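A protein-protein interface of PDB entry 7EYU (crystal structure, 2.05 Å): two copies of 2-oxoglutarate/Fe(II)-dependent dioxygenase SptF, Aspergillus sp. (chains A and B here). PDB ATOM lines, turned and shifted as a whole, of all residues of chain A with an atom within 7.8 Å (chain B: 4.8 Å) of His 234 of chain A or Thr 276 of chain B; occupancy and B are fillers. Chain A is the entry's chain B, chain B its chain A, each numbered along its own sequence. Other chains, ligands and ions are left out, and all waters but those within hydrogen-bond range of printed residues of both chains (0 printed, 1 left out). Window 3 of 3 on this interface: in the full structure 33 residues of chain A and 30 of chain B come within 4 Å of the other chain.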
ATOM      1  N   ASN A  73      -6.535  17.059 -28.865  1.00  0.00           N
ATOM      2  CA  ASN A  73      -5.586  15.954 -29.004  1.00  0.00           C
ATOM      3  C   ASN A  73      -6.042  14.964 -30.070  1.00  0.00           C
ATOM      4  O   ASN A  73      -5.901  13.749 -29.915  1.00  0.00           O
ATOM      5  CB  ASN A  73      -5.373  15.240 -27.677  1.00  0.00           C
ATOM      6  CG  ASN A  73      -3.941  15.205 -27.276  1.00  0.00           C
ATOM      7  OD1 ASN A  73      -3.040  15.461 -28.081  1.00  0.00           O
ATOM      8  ND2 ASN A  73      -3.702  14.902 -26.007  1.00  0.00           N
ATOM      9  N   LEU A  74      -6.588  15.492 -31.165  1.00  0.00           N
ATOM     10  CA  LEU A  74      -7.239  14.641 -32.156  1.00  0.00           C
ATOM     11  C   LEU A  74      -6.244  13.754 -32.891  1.00  0.00           C
ATOM     12  O   LEU A  74      -6.581  12.621 -33.254  1.00  0.00           O
ATOM     13  CB  LEU A  74      -8.020  15.504 -33.147  1.00  0.00           C
ATOM     14  CG  LEU A  74      -9.513  15.721 -32.882  1.00  0.00           C
ATOM     15  CD1 LEU A  74      -9.797  15.908 -31.398  1.00  0.00           C
ATOM     16  CD2 LEU A  74     -10.030  16.911 -33.675  1.00  0.00           C
ATOM     17  N   SER A  75      -5.023  14.241 -33.125  1.00  0.00           N
ATOM     18  CA  SER A  75      -4.032  13.430 -33.824  1.00  0.00           C
ATOM     19  C   SER A  75      -3.577  12.251 -32.971  1.00  0.00           C
ATOM     20  O   SER A  75      -3.357  11.151 -33.488  1.00  0.00           O
ATOM     21  CB  SER A  75      -2.836  14.292 -34.228  1.00  0.00           C
ATOM     22  OG  SER A  75      -3.230  15.336 -35.103  1.00  0.00           O
ATOM     23  N   LEU A  76      -3.436  12.464 -31.660  1.00  0.00           N
ATOM     24  CA  LEU A  76      -3.013  11.385 -30.772  1.00  0.00           C
ATOM     25  C   LEU A  76      -4.099  10.328 -30.609  1.00  0.00           C
ATOM     26  O   LEU A  76      -3.789   9.148 -30.411  1.00  0.00           O
ATOM     27  CB  LEU A  76      -2.618  11.960 -29.410  1.00  0.00           C
ATOM     28  CG  LEU A  76      -2.271  10.980 -28.287  1.00  0.00           C
ATOM     29  CD1 LEU A  76      -0.897  10.369 -28.506  1.00  0.00           C
ATOM     30  CD2 LEU A  76      -2.351  11.667 -26.930  1.00  0.00           C
ATOM     31  N   MET A  77      -5.368  10.724 -30.701  1.00  0.00           N
ATOM     32  CA  MET A  77      -6.482   9.822 -30.443  1.00  0.00           C
ATOM     33  C   MET A  77      -7.087   9.220 -31.705  1.00  0.00           C
ATOM     34  O   MET A  77      -7.842   8.248 -31.601  1.00  0.00           O
ATOM     35  CB  MET A  77      -7.582  10.553 -29.660  1.00  0.00           C
ATOM     36  CG  MET A  77      -7.107  11.193 -28.367  1.00  0.00           C
ATOM     37  SD  MET A  77      -6.442   9.997 -27.194  1.00  0.00           S
ATOM     38  CE  MET A  77      -7.883   8.974 -26.898  1.00  0.00           C
ATOM     39  N   GLU A 230      -2.070  23.968 -29.853  1.00  0.00           N
ATOM     40  CA  GLU A 230      -1.777  22.584 -29.512  1.00  0.00           C
ATOM     41  C   GLU A 230      -0.387  22.224 -30.010  1.00  0.00           C
ATOM     42  O   GLU A 230      -0.070  22.439 -31.183  1.00  0.00           O
ATOM     43  CB  GLU A 230      -2.808  21.630 -30.127  1.00  0.00           C
ATOM     44  CG  GLU A 230      -4.083  21.468 -29.323  1.00  0.00           C
ATOM     45  CD  GLU A 230      -5.108  20.610 -30.040  1.00  0.00           C
ATOM     46  OE1 GLU A 230      -4.945  19.371 -30.051  1.00  0.00           O
ATOM     47  OE2 GLU A 230      -6.073  21.175 -30.596  1.00  0.00           O
ATOM     48  N   SER A 231       0.436  21.686 -29.117  1.00  0.00           N
ATOM     49  CA  SER A 231       1.696  21.075 -29.502  1.00  0.00           C
ATOM     50  C   SER A 231       1.490  19.580 -29.719  1.00  0.00           C
ATOM     51  O   SER A 231       0.518  18.988 -29.245  1.00  0.00           O
ATOM     52  CB  SER A 231       2.768  21.316 -28.437  1.00  0.00           C
ATOM     53  OG  SER A 231       3.993  20.698 -28.794  1.00  0.00           O
ATOM     54  N   HIS A 232       2.419  18.969 -30.456  1.00  0.00           N
ATOM     55  CA  HIS A 232       2.298  17.559 -30.801  1.00  0.00           C
ATOM     56  C   HIS A 232       3.571  16.763 -30.539  1.00  0.00           C
ATOM     57  O   HIS A 232       3.680  15.626 -31.009  1.00  0.00           O
ATOM     58  CB  HIS A 232       1.878  17.407 -32.268  1.00  0.00           C
ATOM     59  CG  HIS A 232       0.490  17.893 -32.547  1.00  0.00           C
ATOM     60  ND1 HIS A 232       0.199  19.216 -32.795  1.00  0.00           N
ATOM     61  CD2 HIS A 232      -0.692  17.231 -32.605  1.00  0.00           C
ATOM     62  CE1 HIS A 232      -1.099  19.351 -32.998  1.00  0.00           C
ATOM     63  NE2 HIS A 232      -1.663  18.161 -32.889  1.00  0.00           N
ATOM     64  N   HIS A 233       4.528  17.315 -29.793  1.00  0.00           N
ATOM     65  CA  HIS A 233       5.777  16.616 -29.516  1.00  0.00           C
ATOM     66  C   HIS A 233       5.672  15.658 -28.336  1.00  0.00           C
ATOM     67  O   HIS A 233       6.660  14.997 -27.999  1.00  0.00           O
ATOM     68  CB  HIS A 233       6.893  17.631 -29.276  1.00  0.00           C
ATOM     69  CG  HIS A 233       7.344  18.328 -30.521  1.00  0.00           C
ATOM     70  ND1 HIS A 233       6.623  19.344 -31.106  1.00  0.00           N
ATOM     71  CD2 HIS A 233       8.449  18.165 -31.285  1.00  0.00           C
ATOM     72  CE1 HIS A 233       7.261  19.773 -32.180  1.00  0.00           C
ATOM     73  NE2 HIS A 233       8.372  19.074 -32.311  1.00  0.00           N
ATOM     74  N   HIS A 234       4.509  15.580 -27.704  1.00  0.00           N
ATOM     75  CA  HIS A 234       4.196  14.555 -26.722  1.00  0.00           C
ATOM     76  C   HIS A 234       3.703  13.266 -27.358  1.00  0.00           C
ATOM     77  O   HIS A 234       3.444  12.298 -26.634  1.00  0.00           O
ATOM     78  CB  HIS A 234       3.101  15.051 -25.799  1.00  0.00           C
ATOM     79  CG  HIS A 234       1.803  15.253 -26.511  1.00  0.00           C
ATOM     80  ND1 HIS A 234       1.620  16.257 -27.438  1.00  0.00           N
ATOM     81  CD2 HIS A 234       0.646  14.551 -26.480  1.00  0.00           C
ATOM     82  CE1 HIS A 234       0.394  16.187 -27.921  1.00  0.00           C
ATOM     83  NE2 HIS A 234      -0.218  15.159 -27.359  1.00  0.00           N
ATOM     84  N   LEU A 235       3.477  13.267 -28.668  1.00  0.00           N
ATOM     85  CA  LEU A 235       3.024  12.074 -29.360  1.00  0.00           C
ATOM     86  C   LEU A 235       4.158  11.056 -29.431  1.00  0.00           C
ATOM     87  O   LEU A 235       5.334  11.426 -29.418  1.00  0.00           O
ATOM     88  CB  LEU A 235       2.555  12.416 -30.774  1.00  0.00           C
ATOM     89  CG  LEU A 235       1.100  12.825 -31.026  1.00  0.00           C
ATOM     90  CD1 LEU A 235       0.804  14.137 -30.374  1.00  0.00           C
ATOM     91  CD2 LEU A 235       0.797  12.913 -32.513  1.00  0.00           C
ATOM     92  N   PRO A 236       3.833   9.764 -29.504  1.00  0.00           N
ATOM     93  CA  PRO A 236       4.883   8.758 -29.687  1.00  0.00           C
ATOM     94  C   PRO A 236       5.621   8.971 -30.999  1.00  0.00           C
ATOM     95  O   PRO A 236       5.072   9.495 -31.970  1.00  0.00           O
ATOM     96  CB  PRO A 236       4.113   7.432 -29.685  1.00  0.00           C
ATOM     97  CG  PRO A 236       2.841   7.735 -28.965  1.00  0.00           C
ATOM     98  CD  PRO A 236       2.508   9.152 -29.319  1.00  0.00           C
ATOM     99  N   ARG A 237       6.889   8.553 -31.017  1.00  0.00           N
ATOM    100  CA  ARG A 237       7.723   8.812 -32.187  1.00  0.00           C
ATOM    101  C   ARG A 237       7.315   7.936 -33.363  1.00  0.00           C
ATOM    102  O   ARG A 237       7.368   8.385 -34.514  1.00  0.00           O
ATOM    103  CB  ARG A 237       9.199   8.595 -31.848  1.00  0.00           C
ATOM    104  CG  ARG A 237       9.728   9.416 -30.670  1.00  0.00           C
ATOM    105  CD  ARG A 237       8.964  10.715 -30.478  1.00  0.00           C
ATOM    106  NE  ARG A 237       9.495  11.778 -31.318  1.00  0.00           N
ATOM    107  CZ  ARG A 237       8.992  13.005 -31.370  1.00  0.00           C
ATOM    108  NH1 ARG A 237       7.946  13.333 -30.622  1.00  0.00           N
ATOM    109  NH2 ARG A 237       9.543  13.913 -32.165  1.00  0.00           N
ATOM    110  N   MET A 239       4.396   7.273 -34.008  1.00  0.00           N
ATOM    111  CA  MET A 239       3.236   7.971 -34.550  1.00  0.00           C
ATOM    112  C   MET A 239       3.650   9.117 -35.464  1.00  0.00           C
ATOM    113  O   MET A 239       2.912   9.466 -36.393  1.00  0.00           O
ATOM    114  CB  MET A 239       2.363   8.487 -33.408  1.00  0.00           C
ATOM    115  CG  MET A 239       0.886   8.539 -33.728  1.00  0.00           C
ATOM    116  SD  MET A 239      -0.103   9.085 -32.323  1.00  0.00           S
ATOM    117  CE  MET A 239      -0.661   7.515 -31.670  1.00  0.00           C
ATOM    118  N   VAL A 240       4.818   9.709 -35.222  1.00  0.00           N
ATOM    119  CA  VAL A 240       5.295  10.798 -36.067  1.00  0.00           C
ATOM    120  C   VAL A 240       5.871  10.256 -37.369  1.00  0.00           C
ATOM    121  O   VAL A 240       5.703  10.860 -38.435  1.00  0.00           O
ATOM    122  CB  VAL A 240       6.324  11.647 -35.298  1.00  0.00           C
ATOM    123  CG1 VAL A 240       6.892  12.745 -36.187  1.00  0.00           C
ATOM    124  CG2 VAL A 240       5.693  12.235 -34.045  1.00  0.00           C
ATOM    125  N   PHE A 253       7.030  19.362 -36.647  1.00  0.00           N
ATOM    126  CA  PHE A 253       8.241  18.551 -36.643  1.00  0.00           C
ATOM    127  C   PHE A 253       9.217  18.930 -37.749  1.00  0.00           C
ATOM    128  O   PHE A 253      10.207  18.222 -37.955  1.00  0.00           O
ATOM    129  CB  PHE A 253       7.882  17.069 -36.750  1.00  0.00           C
ATOM    130  CG  PHE A 253       7.050  16.566 -35.609  1.00  0.00           C
ATOM    131  CD1 PHE A 253       7.642  16.212 -34.409  1.00  0.00           C
ATOM    132  CD2 PHE A 253       5.677  16.455 -35.733  1.00  0.00           C
ATOM    133  CE1 PHE A 253       6.880  15.753 -33.356  1.00  0.00           C
ATOM    134  CE2 PHE A 253       4.908  15.996 -34.682  1.00  0.00           C
ATOM    135  CZ  PHE A 253       5.511  15.647 -33.492  1.00  0.00           C
ATOM    136  N   ARG B 237      16.541  14.271 -23.576  1.00  0.00           N
ATOM    137  CA  ARG B 237      15.566  14.530 -22.518  1.00  0.00           C
ATOM    138  C   ARG B 237      16.224  14.596 -21.149  1.00  0.00           C
ATOM    139  O   ARG B 237      15.696  15.254 -20.244  1.00  0.00           O
ATOM    140  CB  ARG B 237      14.460  13.473 -22.529  1.00  0.00           C
ATOM    141  CG  ARG B 237      13.673  13.427 -23.825  1.00  0.00           C
ATOM    142  CD  ARG B 237      13.231  14.826 -24.239  1.00  0.00           C
ATOM    143  NE  ARG B 237      11.923  15.200 -23.701  1.00  0.00           N
ATOM    144  CZ  ARG B 237      11.307  16.343 -23.986  1.00  0.00           C
ATOM    145  NH1 ARG B 237      11.880  17.211 -24.805  1.00  0.00           N
ATOM    146  NH2 ARG B 237      10.116  16.616 -23.471  1.00  0.00           N
ATOM    147  N   ALA B 267      -0.957  20.378 -24.527  1.00  0.00           N
ATOM    148  CA  ALA B 267      -1.012  18.934 -24.754  1.00  0.00           C
ATOM    149  C   ALA B 267      -2.490  18.567 -24.793  1.00  0.00           C
ATOM    150  O   ALA B 267      -3.071  18.115 -23.803  1.00  0.00           O
ATOM    151  CB  ALA B 267      -0.275  18.166 -23.666  1.00  0.00           C
ATOM    152  N   GLY B 268      -3.105  18.767 -25.952  1.00  0.00           N
ATOM    153  CA  GLY B 268      -4.539  18.611 -26.055  1.00  0.00           C
ATOM    154  C   GLY B 268      -5.223  19.750 -25.334  1.00  0.00           C
ATOM    155  O   GLY B 268      -5.098  20.910 -25.737  1.00  0.00           O
ATOM    156  N   LEU B 272       1.626  20.532 -21.614  1.00  0.00           N
ATOM    157  CA  LEU B 272       2.578  19.713 -22.359  1.00  0.00           C
ATOM    158  C   LEU B 272       3.546  18.999 -21.425  1.00  0.00           C
ATOM    159  O   LEU B 272       3.910  17.842 -21.665  1.00  0.00           O
ATOM    160  CB  LEU B 272       3.338  20.578 -23.367  1.00  0.00           C
ATOM    161  CG  LEU B 272       4.542  19.941 -24.067  1.00  0.00           C
ATOM    162  CD1 LEU B 272       4.118  18.736 -24.896  1.00  0.00           C
ATOM    163  CD2 LEU B 272       5.261  20.964 -24.931  1.00  0.00           C
ATOM    164  N   GLU B 273       3.968  19.672 -20.351  1.00  0.00           N
ATOM    165  CA  GLU B 273       4.900  19.055 -19.413  1.00  0.00           C
ATOM    166  C   GLU B 273       4.258  17.900 -18.657  1.00  0.00           C
ATOM    167  O   GLU B 273       4.957  16.968 -18.246  1.00  0.00           O
ATOM    168  CB  GLU B 273       5.429  20.106 -18.437  1.00  0.00           C
ATOM    169  CG  GLU B 273       4.351  20.828 -17.640  1.00  0.00           C
ATOM    170  CD  GLU B 273       3.834  22.073 -18.338  1.00  0.00           C
ATOM    171  OE1 GLU B 273       3.756  22.075 -19.584  1.00  0.00           O
ATOM    172  OE2 GLU B 273       3.508  23.053 -17.636  1.00  0.00           O
ATOM    173  N   ASP B 274       2.937  17.939 -18.464  1.00  0.00           N
ATOM    174  CA  ASP B 274       2.261  16.841 -17.782  1.00  0.00           C
ATOM    175  C   ASP B 274       2.207  15.598 -18.661  1.00  0.00           C
ATOM    176  O   ASP B 274       2.382  14.476 -18.172  1.00  0.00           O
ATOM    177  CB  ASP B 274       0.853  17.264 -17.367  1.00  0.00           C
ATOM    178  CG  ASP B 274       0.855  18.229 -16.198  1.00  0.00           C
ATOM    179  OD1 ASP B 274       1.789  18.161 -15.372  1.00  0.00           O
ATOM    180  OD2 ASP B 274      -0.078  19.055 -16.105  1.00  0.00           O
ATOM    181  N   ALA B 275       1.966  15.776 -19.960  1.00  0.00           N
ATOM    182  CA  ALA B 275       1.891  14.656 -20.888  1.00  0.00           C
ATOM    183  C   ALA B 275       3.253  14.073 -21.232  1.00  0.00           C
ATOM    184  O   ALA B 275       3.312  12.970 -21.787  1.00  0.00           O
ATOM    185  CB  ALA B 275       1.177  15.086 -22.172  1.00  0.00           C
ATOM    186  N   THR B 276       4.341  14.776 -20.927  1.00  0.00           N
ATOM    187  CA  THR B 276       5.687  14.289 -21.193  1.00  0.00           C
ATOM    188  C   THR B 276       6.391  13.779 -19.943  1.00  0.00           C
ATOM    189  O   THR B 276       7.563  13.399 -20.022  1.00  0.00           O
ATOM    190  CB  THR B 276       6.534  15.389 -21.843  1.00  0.00           C
ATOM    191  OG1 THR B 276       6.415  16.601 -21.086  1.00  0.00           O
ATOM    192  CG2 THR B 276       6.075  15.641 -23.272  1.00  0.00           C
ATOM    193  N   GLY B 277       5.710  13.759 -18.801  1.00  0.00           N
ATOM    194  CA  GLY B 277       6.348  13.332 -17.564  1.00  0.00           C
ATOM    195  C   GLY B 277       7.493  14.226 -17.146  1.00  0.00           C
ATOM    196  O   GLY B 277       8.511  13.736 -16.642  1.00  0.00           O
ATOM    197  N   LEU B 278       7.352  15.532 -17.348  1.00  0.00           N
ATOM    198  CA  LEU B 278       8.420  16.480 -17.052  1.00  0.00           C
ATOM    199  C   LEU B 278       8.271  17.086 -15.660  1.00  0.00           C
ATOM    200  O   LEU B 278       7.242  16.919 -15.007  1.00  0.00           O
ATOM    201  CB  LEU B 278       8.448  17.589 -18.106  1.00  0.00           C
ATOM    202  CG  LEU B 278       9.729  18.417 -18.192  1.00  0.00           C
ATOM    203  CD1 LEU B 278      10.923  17.533 -18.494  1.00  0.00           C
ATOM    204  CD2 LEU B 278       9.588  19.494 -19.253  1.00  0.00           C
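Position printed for both chains: 237. Of the 5 pairs that touch across the chains among the printed residues, none has its exchanged pair printed and touching as well.
His 234 of chain A touches two residues of chain B. Gly 277 of chain B touches none of the printed residues of chain A. Printed residues of chain B within 4 Å of Glu 230 of chain A: Gly 268. Printed residues of chain B within 4 Å of Asn 73 of chain A: Ala 267 and Gly 268. Printed residues of chain A within 4 Å of Leu 272 of chain B: His 234 (3.9 Å). Of the printed residues of chain A, Ala 267 of chain B touches Asn 73 (3.9 Å). Printed residues of chain A within 4 Å of Gly 268 of chain B: Asn 73 (3.7 Å) and Glu 230 (3.8 Å). Asp 274 of chain B touches none of the printed residues of chain A. Met 77 of chain A touches none of the printed residues of chain B. The nearest residue of chain A that does not touch Thr 276 of chain B is His 233 of chain A (4.8 Å). The nearest printed residue of chain A that does not touch Leu 272 of chain B is Ser 231 of chain A (4.1 Å).
The backbone NH (N) of Asn 73 of chain A sits at hydrogen-bond distance from the side-chain carboxylate (OE1) of Glu 230 of chain A, 3.0 Å away. A ring nitrogen (NE2) of His 234 of chain A is in hydrogen-bond range of the side-chain amide oxygen (OD1) of Asn 73 of chain A (2.9 Å). O of Ser 231 of chain A sits close to ND1 of His 234 of chain A. The backbone carbonyl oxygen (O) of Leu 272 of chain B is in hydrogen-bond range of the side-chain hydroxyl (OG1) of Thr 276 of chain B, 2.9 Å away. The backbone carbonyl oxygen (O) of Glu 273 of chain B lies within hydrogen-bond range of the side-chain hydroxyl (OG1) of Thr 276 of chain B (3.2 Å).
Printed residues of chain B that touch a printed residue of chain A: Ala 267, Gly 268, Leu 272 and Thr 276. Of the 16 printed residues of chain A, 3 touch a printed residue of chain B. Printed residues of chain A that touch a printed residue of chain B: Asn 73, Glu 230 and His 234. Hydrophobic or aromatic side chains of chain A within 4 Å of the printed part of chain B: His 234.
Among the printed residues, pairs that only touch across the chains: Asn 73 of chain A with Ala 267 of chain B (3.9 Å), Asn 73 of chain A with Gly 268 of chain B (3.7 Å), Glu 230 of chain A with Gly 268 of chain B (3.8 Å), His 234 of chain A with Leu 272 of chain B (3.9 Å) and His 234 of chain A with Thr 276 of chain B (3.9 Å).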
